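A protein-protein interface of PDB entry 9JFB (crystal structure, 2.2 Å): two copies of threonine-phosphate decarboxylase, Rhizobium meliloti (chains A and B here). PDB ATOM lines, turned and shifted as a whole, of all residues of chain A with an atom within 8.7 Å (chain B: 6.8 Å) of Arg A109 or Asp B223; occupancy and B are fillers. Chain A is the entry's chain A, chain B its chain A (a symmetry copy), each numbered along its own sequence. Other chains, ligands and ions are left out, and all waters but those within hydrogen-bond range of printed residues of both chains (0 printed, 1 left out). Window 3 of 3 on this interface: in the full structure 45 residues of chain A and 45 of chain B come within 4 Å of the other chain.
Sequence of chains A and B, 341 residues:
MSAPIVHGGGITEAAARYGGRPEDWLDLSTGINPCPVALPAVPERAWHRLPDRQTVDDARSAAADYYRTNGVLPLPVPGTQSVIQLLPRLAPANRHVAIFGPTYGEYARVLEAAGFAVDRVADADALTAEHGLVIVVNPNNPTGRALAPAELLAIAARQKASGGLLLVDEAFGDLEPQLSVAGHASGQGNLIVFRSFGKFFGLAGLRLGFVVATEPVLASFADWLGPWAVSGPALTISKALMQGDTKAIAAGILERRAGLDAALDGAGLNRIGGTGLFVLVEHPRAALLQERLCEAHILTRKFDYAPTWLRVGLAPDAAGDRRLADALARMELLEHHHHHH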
ATOM      1  N   PRO A   4     -28.764 -22.950   7.009  1.00  0.00           N
ATOM      2  CA  PRO A   4     -29.517 -22.814   8.263  1.00  0.00           C
ATOM      3  C   PRO A   4     -29.865 -24.163   8.898  1.00  0.00           C
ATOM      4  O   PRO A   4     -29.735 -25.205   8.248  1.00  0.00           O
ATOM      5  CB  PRO A   4     -30.788 -22.064   7.833  1.00  0.00           C
ATOM      6  CG  PRO A   4     -30.387 -21.320   6.591  1.00  0.00           C
ATOM      7  CD  PRO A   4     -29.407 -22.229   5.894  1.00  0.00           C
ATOM      8  N   ILE A   5     -30.277 -24.139  10.163  1.00  0.00           N
ATOM      9  CA  ILE A   5     -30.739 -25.342  10.848  1.00  0.00           C
ATOM     10  C   ILE A   5     -32.169 -25.616  10.412  1.00  0.00           C
ATOM     11  O   ILE A   5     -32.967 -24.686  10.230  1.00  0.00           O
ATOM     12  CB  ILE A   5     -30.654 -25.160  12.374  1.00  0.00           C
ATOM     13  CG1 ILE A   5     -29.212 -24.883  12.823  1.00  0.00           C
ATOM     14  CG2 ILE A   5     -31.273 -26.357  13.110  1.00  0.00           C
ATOM     15  CD1 ILE A   5     -29.124 -24.443  14.284  1.00  0.00           C
ATOM     16  N   VAL A   6     -32.512 -26.889  10.243  1.00  0.00           N
ATOM     17  CA  VAL A   6     -33.886 -27.253   9.898  1.00  0.00           C
ATOM     18  C   VAL A   6     -34.612 -27.519  11.215  1.00  0.00           C
ATOM     19  O   VAL A   6     -34.628 -28.633  11.741  1.00  0.00           O
ATOM     20  CB  VAL A   6     -33.949 -28.435   8.934  1.00  0.00           C
ATOM     21  CG1 VAL A   6     -35.419 -28.781   8.622  1.00  0.00           C
ATOM     22  CG2 VAL A   6     -33.191 -28.102   7.641  1.00  0.00           C
ATOM     23  N   HIS A   7     -35.232 -26.475  11.751  1.00  0.00           N
ATOM     24  CA  HIS A   7     -35.950 -26.596  13.004  1.00  0.00           C
ATOM     25  C   HIS A   7     -37.276 -27.318  12.803  1.00  0.00           C
ATOM     26  O   HIS A   7     -37.789 -27.430  11.691  1.00  0.00           O
ATOM     27  CB  HIS A   7     -36.207 -25.213  13.592  1.00  0.00           C
ATOM     28  CG  HIS A   7     -34.961 -24.502  14.000  1.00  0.00           C
ATOM     29  ND1 HIS A   7     -34.204 -24.897  15.082  1.00  0.00           N
ATOM     30  CD2 HIS A   7     -34.322 -23.441  13.457  1.00  0.00           C
ATOM     31  CE1 HIS A   7     -33.156 -24.100  15.194  1.00  0.00           C
ATOM     32  NE2 HIS A   7     -33.211 -23.201  14.227  1.00  0.00           N
ATOM     33  N   GLN A  81     -34.787 -16.076  20.074  1.00  0.00           N
ATOM     34  CA  GLN A  81     -33.736 -15.915  19.064  1.00  0.00           C
ATOM     35  C   GLN A  81     -33.156 -14.508  19.064  1.00  0.00           C
ATOM     36  O   GLN A  81     -31.948 -14.323  18.848  1.00  0.00           O
ATOM     37  CB  GLN A  81     -34.263 -16.231  17.662  1.00  0.00           C
ATOM     38  CG  GLN A  81     -33.166 -16.142  16.575  1.00  0.00           C
ATOM     39  CD  GLN A  81     -32.128 -17.274  16.672  1.00  0.00           C
ATOM     40  OE1 GLN A  81     -32.387 -18.317  17.265  1.00  0.00           O
ATOM     41  NE2 GLN A  81     -30.961 -17.070  16.075  1.00  0.00           N
ATOM     42  N   ILE A  84     -30.593 -14.515  21.803  1.00  0.00           N
ATOM     43  CA  ILE A  84     -29.504 -15.404  21.402  1.00  0.00           C
ATOM     44  C   ILE A  84     -28.543 -14.653  20.489  1.00  0.00           C
ATOM     45  O   ILE A  84     -27.322 -14.659  20.690  1.00  0.00           O
ATOM     46  CB  ILE A  84     -30.044 -16.672  20.714  1.00  0.00           C
ATOM     47  CG1 ILE A  84     -30.895 -17.501  21.681  1.00  0.00           C
ATOM     48  CG2 ILE A  84     -28.859 -17.513  20.165  1.00  0.00           C
ATOM     49  CD1 ILE A  84     -31.422 -18.819  21.099  1.00  0.00           C
ATOM     50  N   GLN A  85     -29.095 -13.952  19.498  1.00  0.00           N
ATOM     51  CA  GLN A  85     -28.290 -13.183  18.557  1.00  0.00           C
ATOM     52  C   GLN A  85     -27.562 -12.005  19.192  1.00  0.00           C
ATOM     53  O   GLN A  85     -26.663 -11.449  18.564  1.00  0.00           O
ATOM     54  CB  GLN A  85     -29.172 -12.692  17.422  1.00  0.00           C
ATOM     55  CG  GLN A  85     -29.148 -13.657  16.295  1.00  0.00           C
ATOM     56  CD  GLN A  85     -30.405 -13.668  15.491  1.00  0.00           C
ATOM     57  OE1 GLN A  85     -30.606 -14.574  14.677  1.00  0.00           O
ATOM     58  NE2 GLN A  85     -31.268 -12.665  15.696  1.00  0.00           N
ATOM     59  N   PRO A  88     -23.300 -12.614  21.284  1.00  0.00           N
ATOM     60  CA  PRO A  88     -21.944 -12.179  20.900  1.00  0.00           C
ATOM     61  C   PRO A  88     -21.521 -10.848  21.509  1.00  0.00           C
ATOM     62  O   PRO A  88     -20.319 -10.615  21.664  1.00  0.00           O
ATOM     63  CB  PRO A  88     -22.018 -12.097  19.368  1.00  0.00           C
ATOM     64  CG  PRO A  88     -23.039 -13.060  18.993  1.00  0.00           C
ATOM     65  CD  PRO A  88     -24.068 -13.052  20.105  1.00  0.00           C
ATOM     66  N   ILE A  99     -20.899 -24.916  25.838  1.00  0.00           N
ATOM     67  CA  ILE A  99     -22.315 -25.221  25.660  1.00  0.00           C
ATOM     68  C   ILE A  99     -22.577 -26.671  26.074  1.00  0.00           C
ATOM     69  O   ILE A  99     -22.001 -27.603  25.493  1.00  0.00           O
ATOM     70  CB  ILE A  99     -22.767 -24.971  24.214  1.00  0.00           C
ATOM     71  CG1 ILE A  99     -22.471 -23.517  23.810  1.00  0.00           C
ATOM     72  CG2 ILE A  99     -24.255 -25.255  24.086  1.00  0.00           C
ATOM     73  CD1 ILE A  99     -22.993 -23.158  22.435  1.00  0.00           C
ATOM     74  N   TYR A 104     -30.091 -27.328  21.481  1.00  0.00           N
ATOM     75  CA  TYR A 104     -30.592 -26.392  20.479  1.00  0.00           C
ATOM     76  C   TYR A 104     -29.441 -25.723  19.743  1.00  0.00           C
ATOM     77  O   TYR A 104     -28.567 -25.114  20.365  1.00  0.00           O
ATOM     78  CB  TYR A 104     -31.459 -25.345  21.182  1.00  0.00           C
ATOM     79  CG  TYR A 104     -32.241 -24.440  20.267  1.00  0.00           C
ATOM     80  CD1 TYR A 104     -33.162 -24.958  19.354  1.00  0.00           C
ATOM     81  CD2 TYR A 104     -32.101 -23.057  20.349  1.00  0.00           C
ATOM     82  CE1 TYR A 104     -33.896 -24.121  18.533  1.00  0.00           C
ATOM     83  CE2 TYR A 104     -32.836 -22.215  19.537  1.00  0.00           C
ATOM     84  CZ  TYR A 104     -33.727 -22.744  18.633  1.00  0.00           C
ATOM     85  OH  TYR A 104     -34.447 -21.889  17.830  1.00  0.00           O
ATOM     86  N   GLY A 105     -29.427 -25.858  18.424  1.00  0.00           N
ATOM     87  CA  GLY A 105     -28.235 -25.505  17.686  1.00  0.00           C
ATOM     88  C   GLY A 105     -28.025 -24.031  17.401  1.00  0.00           C
ATOM     89  O   GLY A 105     -27.014 -23.681  16.795  1.00  0.00           O
ATOM     90  N   GLU A 106     -28.943 -23.145  17.790  1.00  0.00           N
ATOM     91  CA  GLU A 106     -28.784 -21.742  17.413  1.00  0.00           C
ATOM     92  C   GLU A 106     -27.681 -21.068  18.217  1.00  0.00           C
ATOM     93  O   GLU A 106     -27.028 -20.154  17.716  1.00  0.00           O
ATOM     94  CB  GLU A 106     -30.105 -20.986  17.580  1.00  0.00           C
ATOM     95  CG  GLU A 106     -31.128 -21.293  16.480  1.00  0.00           C
ATOM     96  CD  GLU A 106     -30.716 -20.770  15.102  1.00  0.00           C
ATOM     97  OE1 GLU A 106     -29.887 -19.826  15.031  1.00  0.00           O
ATOM     98  OE2 GLU A 106     -31.228 -21.295  14.080  1.00  0.00           O
ATOM     99  N   TYR A 107     -27.448 -21.522  19.450  1.00  0.00           N
ATOM    100  CA  TYR A 107     -26.377 -20.954  20.259  1.00  0.00           C
ATOM    101  C   TYR A 107     -25.027 -21.096  19.571  1.00  0.00           C
ATOM    102  O   TYR A 107     -24.287 -20.113  19.418  1.00  0.00           O
ATOM    103  CB  TYR A 107     -26.366 -21.612  21.633  1.00  0.00           C
ATOM    104  CG  TYR A 107     -27.578 -21.223  22.444  1.00  0.00           C
ATOM    105  CD1 TYR A 107     -27.651 -19.964  23.025  1.00  0.00           C
ATOM    106  CD2 TYR A 107     -28.654 -22.104  22.620  1.00  0.00           C
ATOM    107  CE1 TYR A 107     -28.747 -19.578  23.769  1.00  0.00           C
ATOM    108  CE2 TYR A 107     -29.777 -21.723  23.368  1.00  0.00           C
ATOM    109  CZ  TYR A 107     -29.812 -20.455  23.936  1.00  0.00           C
ATOM    110  OH  TYR A 107     -30.896 -20.030  24.668  1.00  0.00           O
ATOM    111  N   ALA A 108     -24.693 -22.311  19.128  1.00  0.00           N
ATOM    112  CA  ALA A 108     -23.411 -22.512  18.465  1.00  0.00           C
ATOM    113  C   ALA A 108     -23.381 -21.831  17.101  1.00  0.00           C
ATOM    114  O   ALA A 108     -22.361 -21.250  16.717  1.00  0.00           O
ATOM    115  CB  ALA A 108     -23.112 -24.009  18.325  1.00  0.00           C
ATOM    116  N   ARG A 109     -24.479 -21.899  16.346  1.00  0.00           N
ATOM    117  CA  ARG A 109     -24.505 -21.242  15.041  1.00  0.00           C
ATOM    118  C   ARG A 109     -24.215 -19.745  15.174  1.00  0.00           C
ATOM    119  O   ARG A 109     -23.349 -19.195  14.476  1.00  0.00           O
ATOM    120  CB  ARG A 109     -25.857 -21.475  14.368  1.00  0.00           C
ATOM    121  CG  ARG A 109     -26.104 -20.594  13.155  1.00  0.00           C
ATOM    122  CD  ARG A 109     -27.483 -20.822  12.549  1.00  0.00           C
ATOM    123  NE  ARG A 109     -27.812 -19.824  11.536  1.00  0.00           N
ATOM    124  CZ  ARG A 109     -28.523 -18.721  11.768  1.00  0.00           C
ATOM    125  NH1 ARG A 109     -29.017 -18.446  12.971  1.00  0.00           N
ATOM    126  NH2 ARG A 109     -28.758 -17.877  10.765  1.00  0.00           N
ATOM    127  N   VAL A 110     -24.907 -19.081  16.101  1.00  0.00           N
ATOM    128  CA  VAL A 110     -24.740 -17.645  16.276  1.00  0.00           C
ATOM    129  C   VAL A 110     -23.349 -17.325  16.814  1.00  0.00           C
ATOM    130  O   VAL A 110     -22.676 -16.416  16.318  1.00  0.00           O
ATOM    131  CB  VAL A 110     -25.842 -17.084  17.190  1.00  0.00           C
ATOM    132  CG1 VAL A 110     -25.464 -15.702  17.693  1.00  0.00           C
ATOM    133  CG2 VAL A 110     -27.191 -17.054  16.452  1.00  0.00           C
ATOM    134  N   LEU A 111     -22.886 -18.061  17.827  1.00  0.00           N
ATOM    135  CA  LEU A 111     -21.621 -17.667  18.442  1.00  0.00           C
ATOM    136  C   LEU A 111     -20.432 -17.958  17.525  1.00  0.00           C
ATOM    137  O   LEU A 111     -19.497 -17.153  17.453  1.00  0.00           O
ATOM    138  CB  LEU A 111     -21.467 -18.339  19.799  1.00  0.00           C
ATOM    139  CG  LEU A 111     -22.372 -17.660  20.821  1.00  0.00           C
ATOM    140  CD1 LEU A 111     -22.591 -18.567  22.001  1.00  0.00           C
ATOM    141  CD2 LEU A 111     -21.786 -16.311  21.261  1.00  0.00           C
ATOM    142  N   GLU A 112     -20.462 -19.072  16.781  1.00  0.00           N
ATOM    143  CA  GLU A 112     -19.387 -19.362  15.841  1.00  0.00           C
ATOM    144  C   GLU A 112     -19.405 -18.404  14.656  1.00  0.00           C
ATOM    145  O   GLU A 112     -18.343 -17.987  14.189  1.00  0.00           O
ATOM    146  CB  GLU A 112     -19.468 -20.814  15.371  1.00  0.00           C
ATOM    147  CG  GLU A 112     -19.179 -21.808  16.511  1.00  0.00           C
ATOM    148  CD  GLU A 112     -19.341 -23.269  16.103  1.00  0.00           C
ATOM    149  OE1 GLU A 112     -20.060 -23.545  15.120  1.00  0.00           O
ATOM    150  OE2 GLU A 112     -18.729 -24.145  16.757  1.00  0.00           O
ATOM    151  N   ALA A 113     -20.590 -18.034  14.157  1.00  0.00           N
ATOM    152  CA  ALA A 113     -20.635 -16.995  13.128  1.00  0.00           C
ATOM    153  C   ALA A 113     -19.964 -15.705  13.600  1.00  0.00           C
ATOM    154  O   ALA A 113     -19.373 -14.978  12.798  1.00  0.00           O
ATOM    155  CB  ALA A 113     -22.082 -16.710  12.718  1.00  0.00           C
ATOM    156  N   ALA A 114     -20.031 -15.403  14.888  1.00  0.00           N
ATOM    157  CA  ALA A 114     -19.387 -14.205  15.410  1.00  0.00           C
ATOM    158  C   ALA A 114     -17.925 -14.430  15.778  1.00  0.00           C
ATOM    159  O   ALA A 114     -17.316 -13.555  16.401  1.00  0.00           O
ATOM    160  CB  ALA A 114     -20.154 -13.682  16.625  1.00  0.00           C
ATOM    161  N   GLY A 115     -17.351 -15.581  15.430  1.00  0.00           N
ATOM    162  CA  GLY A 115     -15.939 -15.811  15.669  1.00  0.00           C
ATOM    163  C   GLY A 115     -15.573 -16.347  17.034  1.00  0.00           C
ATOM    164  O   GLY A 115     -14.382 -16.444  17.334  1.00  0.00           O
ATOM    165  N   PHE A 116     -16.544 -16.708  17.873  1.00  0.00           N
ATOM    166  CA  PHE A 116     -16.215 -17.328  19.153  1.00  0.00           C
ATOM    167  C   PHE A 116     -15.847 -18.796  18.965  1.00  0.00           C
ATOM    168  O   PHE A 116     -16.353 -19.477  18.065  1.00  0.00           O
ATOM    169  CB  PHE A 116     -17.384 -17.230  20.132  1.00  0.00           C
ATOM    170  CG  PHE A 116     -17.619 -15.856  20.655  1.00  0.00           C
ATOM    171  CD1 PHE A 116     -18.330 -14.930  19.910  1.00  0.00           C
ATOM    172  CD2 PHE A 116     -17.123 -15.484  21.892  1.00  0.00           C
ATOM    173  CE1 PHE A 116     -18.543 -13.656  20.393  1.00  0.00           C
ATOM    174  CE2 PHE A 116     -17.332 -14.223  22.375  1.00  0.00           C
ATOM    175  CZ  PHE A 116     -18.055 -13.299  21.626  1.00  0.00           C
ATOM    176  N   VAL A 118     -16.375 -22.343  20.375  1.00  0.00           N
ATOM    177  CA  VAL A 118     -17.418 -23.019  21.140  1.00  0.00           C
ATOM    178  C   VAL A 118     -16.923 -24.418  21.502  1.00  0.00           C
ATOM    179  O   VAL A 118     -16.526 -25.194  20.626  1.00  0.00           O
ATOM    180  CB  VAL A 118     -18.735 -23.076  20.348  1.00  0.00           C
ATOM    181  CG1 VAL A 118     -19.765 -23.886  21.085  1.00  0.00           C
ATOM    182  CG2 VAL A 118     -19.252 -21.664  20.103  1.00  0.00           C
ATOM    183  N   ARG A 120     -18.192 -27.892  23.012  1.00  0.00           N
ATOM    184  CA  ARG A 120     -19.297 -28.759  23.409  1.00  0.00           C
ATOM    185  C   ARG A 120     -18.912 -29.534  24.659  1.00  0.00           C
ATOM    186  O   ARG A 120     -17.869 -30.189  24.691  1.00  0.00           O
ATOM    187  CB  ARG A 120     -19.638 -29.735  22.290  1.00  0.00           C
ATOM    188  CG  ARG A 120     -20.047 -29.081  20.997  1.00  0.00           C
ATOM    189  CD  ARG A 120     -19.806 -30.039  19.862  1.00  0.00           C
ATOM    190  NE  ARG A 120     -20.508 -29.660  18.645  1.00  0.00           N
ATOM    191  CZ  ARG A 120     -20.181 -30.099  17.438  1.00  0.00           C
ATOM    192  NH1 ARG A 120     -19.134 -30.891  17.253  1.00  0.00           N
ATOM    193  NH2 ARG A 120     -20.916 -29.733  16.390  1.00  0.00           N
ATOM    194  N   LEU B  75     -38.676  -8.595   2.014  1.00  0.00           N
ATOM    195  CA  LEU B  75     -38.436  -9.387   3.210  1.00  0.00           C
ATOM    196  C   LEU B  75     -39.202  -8.799   4.382  1.00  0.00           C
ATOM    197  O   LEU B  75     -38.971  -7.630   4.738  1.00  0.00           O
ATOM    198  CB  LEU B  75     -36.954  -9.431   3.539  1.00  0.00           C
ATOM    199  CG  LEU B  75     -36.625 -10.322   4.742  1.00  0.00           C
ATOM    200  CD1 LEU B  75     -36.814 -11.812   4.394  1.00  0.00           C
ATOM    201  CD2 LEU B  75     -35.208 -10.049   5.241  1.00  0.00           C
ATOM    202  N   LEU B 218     -30.975  -9.221   0.693  1.00  0.00           N
ATOM    203  CA  LEU B 218     -32.106  -9.772   1.434  1.00  0.00           C
ATOM    204  C   LEU B 218     -31.713 -11.045   2.167  1.00  0.00           C
ATOM    205  O   LEU B 218     -32.151 -11.272   3.303  1.00  0.00           O
ATOM    206  CB  LEU B 218     -33.285 -10.052   0.503  1.00  0.00           C
ATOM    207  CG  LEU B 218     -33.975  -8.836  -0.123  1.00  0.00           C
ATOM    208  CD1 LEU B 218     -35.160  -9.288  -0.966  1.00  0.00           C
ATOM    209  CD2 LEU B 218     -34.405  -7.842   0.949  1.00  0.00           C
ATOM    210  N   ALA B 219     -30.893 -11.892   1.529  1.00  0.00           N
ATOM    211  CA  ALA B 219     -30.438 -13.118   2.181  1.00  0.00           C
ATOM    212  C   ALA B 219     -29.570 -12.791   3.387  1.00  0.00           C
ATOM    213  O   ALA B 219     -29.698 -13.429   4.442  1.00  0.00           O
ATOM    214  CB  ALA B 219     -29.688 -14.009   1.183  1.00  0.00           C
ATOM    215  N   SER B 220     -28.739 -11.749   3.279  1.00  0.00           N
ATOM    216  CA  SER B 220     -27.985 -11.297   4.450  1.00  0.00           C
ATOM    217  C   SER B 220     -28.911 -10.861   5.582  1.00  0.00           C
ATOM    218  O   SER B 220     -28.723 -11.264   6.737  1.00  0.00           O
ATOM    219  CB  SER B 220     -27.031 -10.163   4.075  1.00  0.00           C
ATOM    220  OG  SER B 220     -26.024 -10.632   3.202  1.00  0.00           O
ATOM    221  N   PHE B 221     -29.902 -10.011   5.280  1.00  0.00           N
ATOM    222  CA  PHE B 221     -30.828  -9.577   6.334  1.00  0.00           C
ATOM    223  C   PHE B 221     -31.556 -10.769   6.958  1.00  0.00           C
ATOM    224  O   PHE B 221     -31.709 -10.853   8.185  1.00  0.00           O
ATOM    225  CB  PHE B 221     -31.855  -8.570   5.790  1.00  0.00           C
ATOM    226  CG  PHE B 221     -31.370  -7.142   5.763  1.00  0.00           C
ATOM    227  CD1 PHE B 221     -31.185  -6.435   6.935  1.00  0.00           C
ATOM    228  CD2 PHE B 221     -31.134  -6.504   4.559  1.00  0.00           C
ATOM    229  CE1 PHE B 221     -30.746  -5.119   6.912  1.00  0.00           C
ATOM    230  CE2 PHE B 221     -30.695  -5.190   4.523  1.00  0.00           C
ATOM    231  CZ  PHE B 221     -30.497  -4.496   5.694  1.00  0.00           C
ATOM    232  N   ALA B 222     -32.046 -11.686   6.116  1.00  0.00           N
ATOM    233  CA  ALA B 222     -32.756 -12.858   6.618  1.00  0.00           C
ATOM    234  C   ALA B 222     -31.885 -13.633   7.598  1.00  0.00           C
ATOM    235  O   ALA B 222     -32.319 -13.966   8.709  1.00  0.00           O
ATOM    236  CB  ALA B 222     -33.185 -13.748   5.446  1.00  0.00           C
ATOM    237  N   ASP B 223     -30.633 -13.895   7.210  1.00  0.00           N
ATOM    238  CA  ASP B 223     -29.721 -14.657   8.063  1.00  0.00           C
ATOM    239  C   ASP B 223     -29.462 -13.934   9.373  1.00  0.00           C
ATOM    240  O   ASP B 223     -29.508 -14.549  10.444  1.00  0.00           O
ATOM    241  CB  ASP B 223     -28.402 -14.907   7.326  1.00  0.00           C
ATOM    242  CG  ASP B 223     -27.431 -15.737   8.137  1.00  0.00           C
ATOM    243  OD1 ASP B 223     -27.650 -16.969   8.259  1.00  0.00           O
ATOM    244  OD2 ASP B 223     -26.456 -15.151   8.657  1.00  0.00           O
ATOM    245  N   TRP B 224     -29.209 -12.622   9.307  1.00  0.00           N
ATOM    246  CA  TRP B 224     -28.969 -11.841  10.518  1.00  0.00           C
ATOM    247  C   TRP B 224     -30.179 -11.814  11.444  1.00  0.00           C
ATOM    248  O   TRP B 224     -30.020 -11.708  12.667  1.00  0.00           O
ATOM    249  CB  TRP B 224     -28.572 -10.405  10.151  1.00  0.00           C
ATOM    250  CG  TRP B 224     -27.267 -10.279   9.431  1.00  0.00           C
ATOM    251  CD1 TRP B 224     -26.187 -11.109   9.538  1.00  0.00           C
ATOM    252  CD2 TRP B 224     -26.896  -9.256   8.489  1.00  0.00           C
ATOM    253  NE1 TRP B 224     -25.177 -10.674   8.720  1.00  0.00           N
ATOM    254  CE2 TRP B 224     -25.584  -9.541   8.064  1.00  0.00           C
ATOM    255  CE3 TRP B 224     -27.551  -8.133   7.961  1.00  0.00           C
ATOM    256  CZ2 TRP B 224     -24.908  -8.744   7.135  1.00  0.00           C
ATOM    257  CZ3 TRP B 224     -26.883  -7.348   7.032  1.00  0.00           C
ATOM    258  CH2 TRP B 224     -25.572  -7.655   6.636  1.00  0.00           C
ATOM    259  N   LEU B 225     -31.397 -11.850  10.896  1.00  0.00           N
ATOM    260  CA  LEU B 225     -32.570 -11.730  11.766  1.00  0.00           C
ATOM    261  C   LEU B 225     -32.917 -13.050  12.444  1.00  0.00           C
ATOM    262  O   LEU B 225     -33.506 -13.040  13.533  1.00  0.00           O
ATOM    263  CB  LEU B 225     -33.777 -11.205  10.978  1.00  0.00           C
ATOM    264  CG  LEU B 225     -33.697  -9.708  10.640  1.00  0.00           C
ATOM    265  CD1 LEU B 225     -34.687  -9.354   9.556  1.00  0.00           C
ATOM    266  CD2 LEU B 225     -33.920  -8.847  11.882  1.00  0.00           C
ATOM    267  N   GLY B 226     -32.548 -14.180  11.832  1.00  0.00           N
ATOM    268  CA  GLY B 226     -32.763 -15.482  12.424  1.00  0.00           C
ATOM    269  C   GLY B 226     -34.168 -16.007  12.194  1.00  0.00           C
ATOM    270  O   GLY B 226     -35.014 -15.345  11.586  1.00  0.00           O
ATOM    271  N   PRO B 227     -34.440 -17.212  12.683  1.00  0.00           N
ATOM    272  CA  PRO B 227     -35.735 -17.849  12.412  1.00  0.00           C
ATOM    273  C   PRO B 227     -36.895 -17.215  13.176  1.00  0.00           C
ATOM    274  O   PRO B 227     -36.746 -16.736  14.305  1.00  0.00           O
ATOM    275  CB  PRO B 227     -35.508 -19.296  12.864  1.00  0.00           C
ATOM    276  CG  PRO B 227     -34.379 -19.197  13.886  1.00  0.00           C
ATOM    277  CD  PRO B 227     -33.482 -18.141  13.319  1.00  0.00           C
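No position is printed for both chains. Of the 6 pairs that touch across the chains among the printed residues, none has its exchanged pair printed and touching as well.
Of the 24 printed residues of chain A, 4 touch a printed residue of chain B. Hydrophobic or aromatic side chains of chain B within 4 Å of the printed part of chain A: Pro B227. Along chain B the printed residues that touch a printed residue of chain A span positions 223 to 227. Among the printed residues, 6 pairs touch across the chains. Among the printed residues, Asp or Glu carboxylates within 4 Å of a Lys or Arg side-chain nitrogen of the other chain: Arg A109 with Asp B223 (2.9 Å).
The side-chain amide nitrogen of Gln A85 is in hydrogen-bond range of the backbone carbonyl oxygen of Trp B224. The backbone NH (N) of Gly B226 lies close to the side-chain amide oxygen (OE1) of Gln A85. The side-chain amide nitrogen (NE2) of Gln A85 is in hydrogen-bond range of the backbone carbonyl oxygen (O) of Leu B225 (3.1 Å). The guanidinium group (NH2) of Arg A109 is in salt-bridge range of the side-chain carboxylate (OD1) of Asp B223, 2.9 Å away.
Among the printed residues, pairs that only touch across the chains: Gln A81 with Pro B227 (3.7 Å) and Glu A106 with Pro B227 (3.8 Å).
Arg A109 touches just one residue of chain B: Asp B223. Asp B223 touches just one residue of chain A: Arg A109. Printed residues of chain B within 4 Å of Gln A81: Pro B227 (3.7 Å). Printed residues of chain A within 4 Å of Leu B225: Gln A85. Of the printed residues of chain A, Pro B227 touches Gln A81 and Glu A106. Val A118 touches none of the printed residues of chain B. The nearest residue of chain B that does not touch Arg A109 is Pro B227 (4.5 Å). The nearest residue of chain A that does not touch Asp B223 is Gln A85 (4.4 Å).
The side-chain carboxylate of Glu A106 is in salt-bridge range of the guanidinium group of Arg A109. OE1 of Glu A106 lies within hydrogen-bond range of NE2 of Gln A81 (3.1 Å). NE2 of Gln A81 sits at hydrogen-bond distance from OE1 of Gln A85 (2.9 Å). A ring nitrogen (NE2) of His A7 sits at hydrogen-bond distance from the side-chain carboxylate of Glu A106, at 2.8 Å.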
